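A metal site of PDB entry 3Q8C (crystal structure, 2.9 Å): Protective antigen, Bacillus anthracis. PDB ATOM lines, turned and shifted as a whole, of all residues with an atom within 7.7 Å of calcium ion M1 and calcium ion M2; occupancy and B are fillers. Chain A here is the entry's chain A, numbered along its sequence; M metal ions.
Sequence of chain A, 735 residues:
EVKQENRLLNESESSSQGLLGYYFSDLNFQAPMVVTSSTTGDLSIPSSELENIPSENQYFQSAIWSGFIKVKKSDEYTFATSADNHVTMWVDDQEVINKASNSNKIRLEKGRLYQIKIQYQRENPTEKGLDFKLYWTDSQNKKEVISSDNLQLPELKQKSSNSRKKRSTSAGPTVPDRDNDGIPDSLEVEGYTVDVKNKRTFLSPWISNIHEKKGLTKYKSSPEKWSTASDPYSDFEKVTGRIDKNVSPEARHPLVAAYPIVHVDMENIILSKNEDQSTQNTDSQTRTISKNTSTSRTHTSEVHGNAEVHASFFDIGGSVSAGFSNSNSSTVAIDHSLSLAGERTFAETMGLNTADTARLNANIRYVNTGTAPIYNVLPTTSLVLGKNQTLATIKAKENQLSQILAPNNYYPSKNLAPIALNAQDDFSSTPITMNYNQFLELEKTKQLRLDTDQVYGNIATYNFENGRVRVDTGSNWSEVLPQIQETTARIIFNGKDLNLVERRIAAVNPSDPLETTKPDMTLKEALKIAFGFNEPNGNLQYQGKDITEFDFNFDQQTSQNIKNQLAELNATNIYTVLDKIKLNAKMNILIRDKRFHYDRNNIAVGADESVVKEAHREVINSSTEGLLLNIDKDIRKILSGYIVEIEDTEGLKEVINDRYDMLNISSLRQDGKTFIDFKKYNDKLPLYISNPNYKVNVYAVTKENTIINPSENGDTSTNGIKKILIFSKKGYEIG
N of Asp 185 sits at hydrogen-bond distance from O of Pro 176 (3.0 Å).
OD2 of Asp 185 is in salt-bridge range of NH1 of Arg 178 (3.5 Å).
OG1 of Thr 228 sits at hydrogen-bond distance from N of Ser 222, at 2.9 Å.
N of Thr 228 lies within hydrogen-bond range of OD1 of Asp 235 (2.9 Å).
O of Pro 223 is in hydrogen-bond range of N of Asp 179 (3.3 Å).
OG of Ser 222 sits close to N of Lys 225, 3.2 Å away.
The backbone NH of Asn 180 sits close to the side-chain carboxylate of Asp 177.
N of Glu 224 lies close to OG of Ser 222, at 3.1 Å.
Merely in contact with calcium ion M1: Asp 185 (3.5 Å) and Pro 223 (3.8 Å).
Thr 228 touches calcium ion M2.
Within 4 Å of calcium ion M2: Asp 179, Asp 181, Glu 188, Ser 222, Lys 225, Thr 228 and Asp 235.
The nearest printed residue that does not touch calcium ion M2 is Trp 226 (4.1 Å).
Calcium ion M1 is bound by OD1 of Asp 179 (2.5 Å), OE1 of Glu 188 (2.6 Å), O of Ile 183 (2.6 Å), OD1 of Asp 177 (2.6 Å) and OD1 of Asp 181 (2.7 Å).
Calcium ion M2 is bound by OD2 of Asp 181 (2.3 Å), O of Ser 222 (2.4 Å), OD2 of Asp 179 (2.4 Å), OD2 of Asp 235 (2.5 Å), OE2 of Glu 188 (2.5 Å), O of Lys 225 (2.6 Å) and OE1 of Glu 188 (2.8 Å).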
ATOM      1  N   PRO A 176     -13.694 -18.678   9.932  1.00  0.00           N
ATOM      2  CA  PRO A 176     -12.452 -19.462   9.830  1.00  0.00           C
ATOM      3  C   PRO A 176     -12.489 -20.780  10.606  1.00  0.00           C
ATOM      4  O   PRO A 176     -12.737 -20.824  11.812  1.00  0.00           O
ATOM      5  CB  PRO A 176     -11.384 -18.513  10.398  1.00  0.00           C
ATOM      6  CG  PRO A 176     -12.005 -17.143  10.329  1.00  0.00           C
ATOM      7  CD  PRO A 176     -13.472 -17.364  10.551  1.00  0.00           C
ATOM      8  N   ASP A 177     -12.242 -21.851   9.868  1.00  0.00           N
ATOM      9  CA  ASP A 177     -12.344 -23.205  10.387  1.00  0.00           C
ATOM     10  C   ASP A 177     -11.344 -24.022   9.594  1.00  0.00           C
ATOM     11  O   ASP A 177     -11.717 -24.830   8.730  1.00  0.00           O
ATOM     12  CB  ASP A 177     -13.779 -23.709  10.187  1.00  0.00           C
ATOM     13  CG  ASP A 177     -14.028 -25.046  10.832  1.00  0.00           C
ATOM     14  OD1 ASP A 177     -13.214 -25.491  11.649  1.00  0.00           O
ATOM     15  OD2 ASP A 177     -15.059 -25.670  10.520  1.00  0.00           O
ATOM     16  N   ARG A 178     -10.058 -23.800   9.867  1.00  0.00           N
ATOM     17  CA  ARG A 178      -8.982 -24.312   9.029  1.00  0.00           C
ATOM     18  C   ARG A 178      -8.985 -25.812   8.844  1.00  0.00           C
ATOM     19  O   ARG A 178      -8.734 -26.302   7.754  1.00  0.00           O
ATOM     20  CB  ARG A 178      -7.621 -23.909   9.602  1.00  0.00           C
ATOM     21  CG  ARG A 178      -7.310 -22.437   9.471  1.00  0.00           C
ATOM     22  CD  ARG A 178      -6.217 -22.050  10.442  1.00  0.00           C
ATOM     23  NE  ARG A 178      -5.195 -21.227   9.806  1.00  0.00           N
ATOM     24  CZ  ARG A 178      -5.413 -20.017   9.302  1.00  0.00           C
ATOM     25  NH1 ARG A 178      -6.625 -19.466   9.358  1.00  0.00           N
ATOM     26  NH2 ARG A 178      -4.407 -19.346   8.743  1.00  0.00           N
ATOM     27  N   ASP A 179      -9.237 -26.553   9.915  1.00  0.00           N
ATOM     28  CA  ASP A 179      -9.198 -28.008   9.844  1.00  0.00           C
ATOM     29  C   ASP A 179     -10.549 -28.554   9.426  1.00  0.00           C
ATOM     30  O   ASP A 179     -10.665 -29.720   9.050  1.00  0.00           O
ATOM     31  CB  ASP A 179      -8.788 -28.612  11.188  1.00  0.00           C
ATOM     32  CG  ASP A 179      -9.655 -28.149  12.342  1.00  0.00           C
ATOM     33  OD1 ASP A 179     -10.770 -27.663  12.094  1.00  0.00           O
ATOM     34  OD2 ASP A 179      -9.224 -28.271  13.490  1.00  0.00           O
ATOM     35  N   ASN A 180     -11.576 -27.711   9.517  1.00  0.00           N
ATOM     36  CA  ASN A 180     -12.914 -28.086   9.072  1.00  0.00           C
ATOM     37  C   ASN A 180     -13.569 -29.132   9.989  1.00  0.00           C
ATOM     38  O   ASN A 180     -14.273 -30.033   9.519  1.00  0.00           O
ATOM     39  CB  ASN A 180     -12.870 -28.602   7.637  1.00  0.00           C
ATOM     40  CG  ASN A 180     -14.229 -28.647   6.993  1.00  0.00           C
ATOM     41  OD1 ASN A 180     -15.029 -27.719   7.137  1.00  0.00           O
ATOM     42  ND2 ASN A 180     -14.514 -29.728   6.282  1.00  0.00           N
ATOM     43  N   ASP A 181     -13.333 -29.010  11.295  1.00  0.00           N
ATOM     44  CA  ASP A 181     -14.025 -29.869  12.254  1.00  0.00           C
ATOM     45  C   ASP A 181     -15.327 -29.204  12.684  1.00  0.00           C
ATOM     46  O   ASP A 181     -16.223 -29.874  13.191  1.00  0.00           O
ATOM     47  CB  ASP A 181     -13.156 -30.201  13.472  1.00  0.00           C
ATOM     48  CG  ASP A 181     -12.463 -28.987  14.085  1.00  0.00           C
ATOM     49  OD1 ASP A 181     -12.832 -27.822  13.822  1.00  0.00           O
ATOM     50  OD2 ASP A 181     -11.531 -29.215  14.855  1.00  0.00           O
ATOM     51  N   GLY A 182     -15.415 -27.897  12.456  1.00  0.00           N
ATOM     52  CA  GLY A 182     -16.619 -27.143  12.759  1.00  0.00           C
ATOM     53  C   GLY A 182     -16.387 -26.069  13.809  1.00  0.00           C
ATOM     54  O   GLY A 182     -16.936 -24.980  13.709  1.00  0.00           O
ATOM     55  N   ILE A 183     -15.590 -26.394  14.824  1.00  0.00           N
ATOM     56  CA  ILE A 183     -15.223 -25.428  15.844  1.00  0.00           C
ATOM     57  C   ILE A 183     -14.348 -24.357  15.211  1.00  0.00           C
ATOM     58  O   ILE A 183     -13.282 -24.677  14.699  1.00  0.00           O
ATOM     59  CB  ILE A 183     -14.424 -26.066  16.992  1.00  0.00           C
ATOM     60  CG1 ILE A 183     -15.213 -27.193  17.649  1.00  0.00           C
ATOM     61  CG2 ILE A 183     -14.069 -25.033  18.046  1.00  0.00           C
ATOM     62  CD1 ILE A 183     -14.400 -28.020  18.616  1.00  0.00           C
ATOM     63  N   PRO A 184     -14.805 -23.081  15.232  1.00  0.00           N
ATOM     64  CA  PRO A 184     -14.000 -21.982  14.670  1.00  0.00           C
ATOM     65  C   PRO A 184     -12.596 -21.928  15.284  1.00  0.00           C
ATOM     66  O   PRO A 184     -12.399 -22.513  16.346  1.00  0.00           O
ATOM     67  CB  PRO A 184     -14.806 -20.733  15.032  1.00  0.00           C
ATOM     68  CG  PRO A 184     -16.196 -21.202  15.198  1.00  0.00           C
ATOM     69  CD  PRO A 184     -16.082 -22.587  15.775  1.00  0.00           C
ATOM     70  N   ASP A 185     -11.663 -21.253  14.625  1.00  0.00           N
ATOM     71  CA  ASP A 185     -10.273 -21.204  15.064  1.00  0.00           C
ATOM     72  C   ASP A 185     -10.111 -20.479  16.400  1.00  0.00           C
ATOM     73  O   ASP A 185      -9.483 -20.990  17.322  1.00  0.00           O
ATOM     74  CB  ASP A 185      -9.411 -20.522  14.010  1.00  0.00           C
ATOM     75  CG  ASP A 185      -9.381 -21.290  12.700  1.00  0.00           C
ATOM     76  OD1 ASP A 185      -9.755 -22.494  12.693  1.00  0.00           O
ATOM     77  OD2 ASP A 185      -8.974 -20.693  11.674  1.00  0.00           O
ATOM     78  N   SER A 186     -10.691 -19.290  16.499  1.00  0.00           N
ATOM     79  CA  SER A 186     -10.529 -18.489  17.703  1.00  0.00           C
ATOM     80  C   SER A 186     -10.967 -19.263  18.934  1.00  0.00           C
ATOM     81  O   SER A 186     -10.274 -19.233  19.950  1.00  0.00           O
ATOM     82  CB  SER A 186     -11.299 -17.170  17.583  1.00  0.00           C
ATOM     83  OG  SER A 186     -12.658 -17.376  17.239  1.00  0.00           O
ATOM     84  N   GLU A 188     -11.056 -22.521  19.441  1.00  0.00           N
ATOM     85  CA  GLU A 188     -10.234 -23.676  19.762  1.00  0.00           C
ATOM     86  C   GLU A 188      -8.996 -23.256  20.542  1.00  0.00           C
ATOM     87  O   GLU A 188      -8.437 -24.049  21.293  1.00  0.00           O
ATOM     88  CB  GLU A 188      -9.805 -24.397  18.493  1.00  0.00           C
ATOM     89  CG  GLU A 188     -10.945 -25.051  17.746  1.00  0.00           C
ATOM     90  CD  GLU A 188     -10.497 -26.276  16.972  1.00  0.00           C
ATOM     91  OE1 GLU A 188     -10.828 -26.410  15.774  1.00  0.00           O
ATOM     92  OE2 GLU A 188      -9.828 -27.130  17.594  1.00  0.00           O
ATOM     93  N   TYR A 192     -13.043 -23.231  25.288  1.00  0.00           N
ATOM     94  CA  TYR A 192     -14.486 -23.313  25.096  1.00  0.00           C
ATOM     95  C   TYR A 192     -15.072 -24.404  25.983  1.00  0.00           C
ATOM     96  O   TYR A 192     -14.356 -25.294  26.432  1.00  0.00           O
ATOM     97  CB  TYR A 192     -14.824 -23.576  23.622  1.00  0.00           C
ATOM     98  CG  TYR A 192     -14.233 -24.851  23.054  1.00  0.00           C
ATOM     99  CD1 TYR A 192     -12.923 -24.881  22.601  1.00  0.00           C
ATOM    100  CD2 TYR A 192     -14.984 -26.027  22.980  1.00  0.00           C
ATOM    101  CE1 TYR A 192     -12.372 -26.036  22.091  1.00  0.00           C
ATOM    102  CE2 TYR A 192     -14.440 -27.186  22.486  1.00  0.00           C
ATOM    103  CZ  TYR A 192     -13.136 -27.184  22.034  1.00  0.00           C
ATOM    104  OH  TYR A 192     -12.573 -28.337  21.530  1.00  0.00           O
ATOM    105  N   LYS A 220      -9.477 -26.917  25.133  1.00  0.00           N
ATOM    106  CA  LYS A 220      -8.619 -26.312  24.132  1.00  0.00           C
ATOM    107  C   LYS A 220      -8.196 -27.376  23.112  1.00  0.00           C
ATOM    108  O   LYS A 220      -8.162 -28.572  23.429  1.00  0.00           O
ATOM    109  CB  LYS A 220      -7.406 -25.656  24.773  1.00  0.00           C
ATOM    110  CG  LYS A 220      -7.667 -24.259  25.298  1.00  0.00           C
ATOM    111  CD  LYS A 220      -6.511 -23.765  26.159  1.00  0.00           C
ATOM    112  CE  LYS A 220      -6.704 -22.312  26.581  1.00  0.00           C
ATOM    113  NZ  LYS A 220      -5.642 -21.842  27.519  1.00  0.00           N
ATOM    114  N   SER A 221      -7.876 -26.934  21.906  1.00  0.00           N
ATOM    115  CA  SER A 221      -7.533 -27.864  20.818  1.00  0.00           C
ATOM    116  C   SER A 221      -6.937 -27.137  19.605  1.00  0.00           C
ATOM    117  O   SER A 221      -7.046 -25.920  19.477  1.00  0.00           O
ATOM    118  CB  SER A 221      -8.764 -28.683  20.417  1.00  0.00           C
ATOM    119  OG  SER A 221      -9.897 -27.849  20.210  1.00  0.00           O
ATOM    120  N   SER A 222      -6.298 -27.902  18.719  1.00  0.00           N
ATOM    121  CA  SER A 222      -5.588 -27.336  17.561  1.00  0.00           C
ATOM    122  C   SER A 222      -6.539 -26.909  16.449  1.00  0.00           C
ATOM    123  O   SER A 222      -7.287 -27.718  15.937  1.00  0.00           O
ATOM    124  CB  SER A 222      -4.591 -28.350  17.004  1.00  0.00           C
ATOM    125  OG  SER A 222      -4.060 -27.910  15.768  1.00  0.00           O
ATOM    126  N   PRO A 223      -6.492 -25.633  16.059  1.00  0.00           N
ATOM    127  CA  PRO A 223      -7.386 -25.220  14.966  1.00  0.00           C
ATOM    128  C   PRO A 223      -6.905 -25.730  13.608  1.00  0.00           C
ATOM    129  O   PRO A 223      -7.560 -25.467  12.599  1.00  0.00           O
ATOM    130  CB  PRO A 223      -7.326 -23.687  15.016  1.00  0.00           C
ATOM    131  CG  PRO A 223      -6.010 -23.376  15.686  1.00  0.00           C
ATOM    132  CD  PRO A 223      -5.720 -24.513  16.623  1.00  0.00           C
ATOM    133  N   GLU A 224      -5.773 -26.444  13.599  1.00  0.00           N
ATOM    134  CA  GLU A 224      -5.156 -26.974  12.380  1.00  0.00           C
ATOM    135  C   GLU A 224      -5.241 -28.502  12.315  1.00  0.00           C
ATOM    136  O   GLU A 224      -4.861 -29.108  11.314  1.00  0.00           O
ATOM    137  CB  GLU A 224      -3.685 -26.560  12.296  1.00  0.00           C
ATOM    138  CG  GLU A 224      -3.345 -25.212  12.974  1.00  0.00           C
ATOM    139  CD  GLU A 224      -3.524 -24.002  12.058  1.00  0.00           C
ATOM    140  OE1 GLU A 224      -3.733 -22.890  12.596  1.00  0.00           O
ATOM    141  OE2 GLU A 224      -3.428 -24.155  10.814  1.00  0.00           O
ATOM    142  N   LYS A 225      -5.733 -29.117  13.379  1.00  0.00           N
ATOM    143  CA  LYS A 225      -5.931 -30.561  13.390  1.00  0.00           C
ATOM    144  C   LYS A 225      -7.419 -30.893  13.493  1.00  0.00           C
ATOM    145  O   LYS A 225      -8.050 -30.646  14.509  1.00  0.00           O
ATOM    146  CB  LYS A 225      -5.161 -31.187  14.543  1.00  0.00           C
ATOM    147  CG  LYS A 225      -3.739 -30.682  14.634  1.00  0.00           C
ATOM    148  CD  LYS A 225      -2.883 -31.592  15.470  1.00  0.00           C
ATOM    149  CE  LYS A 225      -2.504 -32.797  14.668  1.00  0.00           C
ATOM    150  NZ  LYS A 225      -2.439 -34.002  15.488  1.00  0.00           N
ATOM    151  N   TRP A 226      -7.981 -31.456  12.432  1.00  0.00           N
ATOM    152  CA  TRP A 226      -9.358 -31.912  12.464  1.00  0.00           C
ATOM    153  C   TRP A 226      -9.578 -32.696  13.755  1.00  0.00           C
ATOM    154  O   TRP A 226     -10.584 -32.529  14.452  1.00  0.00           O
ATOM    155  CB  TRP A 226      -9.635 -32.797  11.266  1.00  0.00           C
ATOM    156  CG  TRP A 226     -11.035 -33.308  11.215  1.00  0.00           C
ATOM    157  CD1 TRP A 226     -12.140 -32.598  10.909  1.00  0.00           C
ATOM    158  CD2 TRP A 226     -11.475 -34.651  11.456  1.00  0.00           C
ATOM    159  NE1 TRP A 226     -13.253 -33.407  10.949  1.00  0.00           N
ATOM    160  CE2 TRP A 226     -12.874 -34.673  11.281  1.00  0.00           C
ATOM    161  CE3 TRP A 226     -10.814 -35.844  11.815  1.00  0.00           C
ATOM    162  CZ2 TRP A 226     -13.633 -35.832  11.442  1.00  0.00           C
ATOM    163  CZ3 TRP A 226     -11.574 -36.993  11.972  1.00  0.00           C
ATOM    164  CH2 TRP A 226     -12.972 -36.987  11.787  1.00  0.00           C
ATOM    165  N   SER A 227      -8.625 -33.573  14.045  1.00  0.00           N
ATOM    166  CA  SER A 227      -8.601 -34.282  15.309  1.00  0.00           C
ATOM    167  C   SER A 227      -7.263 -34.007  15.996  1.00  0.00           C
ATOM    168  O   SER A 227      -6.207 -34.319  15.450  1.00  0.00           O
ATOM    169  CB  SER A 227      -8.813 -35.772  15.094  1.00  0.00           C
ATOM    170  OG  SER A 227      -8.303 -36.522  16.174  1.00  0.00           O
ATOM    171  N   THR A 228      -7.320 -33.421  17.194  1.00  0.00           N
ATOM    172  CA  THR A 228      -6.130 -32.900  17.850  1.00  0.00           C
ATOM    173  C   THR A 228      -5.249 -33.984  18.461  1.00  0.00           C
ATOM    174  O   THR A 228      -4.052 -33.780  18.661  1.00  0.00           O
ATOM    175  CB  THR A 228      -6.495 -31.876  18.932  1.00  0.00           C
ATOM    176  OG1 THR A 228      -6.913 -30.664  18.295  1.00  0.00           O
ATOM    177  CG2 THR A 228      -5.311 -31.602  19.834  1.00  0.00           C
ATOM    178  N   SER A 234     -13.371 -36.273  15.268  1.00  0.00           N
ATOM    179  CA  SER A 234     -12.999 -34.844  15.245  1.00  0.00           C
ATOM    180  C   SER A 234     -13.153 -34.156  16.597  1.00  0.00           C
ATOM    181  O   SER A 234     -13.771 -34.664  17.518  1.00  0.00           O
ATOM    182  CB  SER A 234     -13.791 -34.090  14.174  1.00  0.00           C
ATOM    183  OG  SER A 234     -15.172 -34.057  14.471  1.00  0.00           O
ATOM    184  N   ASP A 235     -12.566 -32.973  16.716  1.00  0.00           N
ATOM    185  CA  ASP A 235     -12.600 -32.287  17.979  1.00  0.00           C
ATOM    186  C   ASP A 235     -14.021 -31.806  18.240  1.00  0.00           C
ATOM    187  O   ASP A 235     -14.408 -31.549  19.391  1.00  0.00           O
ATOM    188  CB  ASP A 235     -11.571 -31.151  17.979  1.00  0.00           C
ATOM    189  CG  ASP A 235     -10.157 -31.679  17.818  1.00  0.00           C
ATOM    190  OD1 ASP A 235      -9.853 -32.781  18.352  1.00  0.00           O
ATOM    191  OD2 ASP A 235      -9.348 -31.030  17.147  1.00  0.00           O
ATOM    192  N   PHE A 236     -14.805 -31.732  17.160  1.00  0.00           N
ATOM    193  CA  PHE A 236     -16.207 -31.322  17.238  1.00  0.00           C
ATOM    194  C   PHE A 236     -17.109 -32.529  17.469  1.00  0.00           C
ATOM    195  O   PHE A 236     -18.118 -32.442  18.153  1.00  0.00           O
ATOM    196  CB  PHE A 236     -16.602 -30.615  15.939  1.00  0.00           C
ATOM    197  CG  PHE A 236     -18.010 -30.133  15.901  1.00  0.00           C
ATOM    198  CD1 PHE A 236     -18.377 -28.965  16.554  1.00  0.00           C
ATOM    199  CD2 PHE A 236     -18.971 -30.805  15.163  1.00  0.00           C
ATOM    200  CE1 PHE A 236     -19.688 -28.501  16.498  1.00  0.00           C
ATOM    201  CE2 PHE A 236     -20.285 -30.344  15.098  1.00  0.00           C
ATOM    202  CZ  PHE A 236     -20.642 -29.196  15.756  1.00  0.00           C
ATOM    203  N   PRO A 254     -10.925 -33.531  23.497  1.00  0.00           N
ATOM    204  CA  PRO A 254     -10.147 -33.318  22.259  1.00  0.00           C
ATOM    205  C   PRO A 254      -8.678 -33.711  22.388  1.00  0.00           C
ATOM    206  O   PRO A 254      -8.028 -33.970  21.369  1.00  0.00           O
ATOM    207  CB  PRO A 254     -10.260 -31.813  22.043  1.00  0.00           C
ATOM    208  CG  PRO A 254     -11.568 -31.449  22.637  1.00  0.00           C
ATOM    209  CD  PRO A 254     -11.764 -32.361  23.822  1.00  0.00           C
HETATM  210 CA    CA M   1     -11.251 -25.626  13.379  1.00  0.00          CA
HETATM  211 CA    CA M   2      -9.426 -28.888  15.843  1.00  0.00          CA
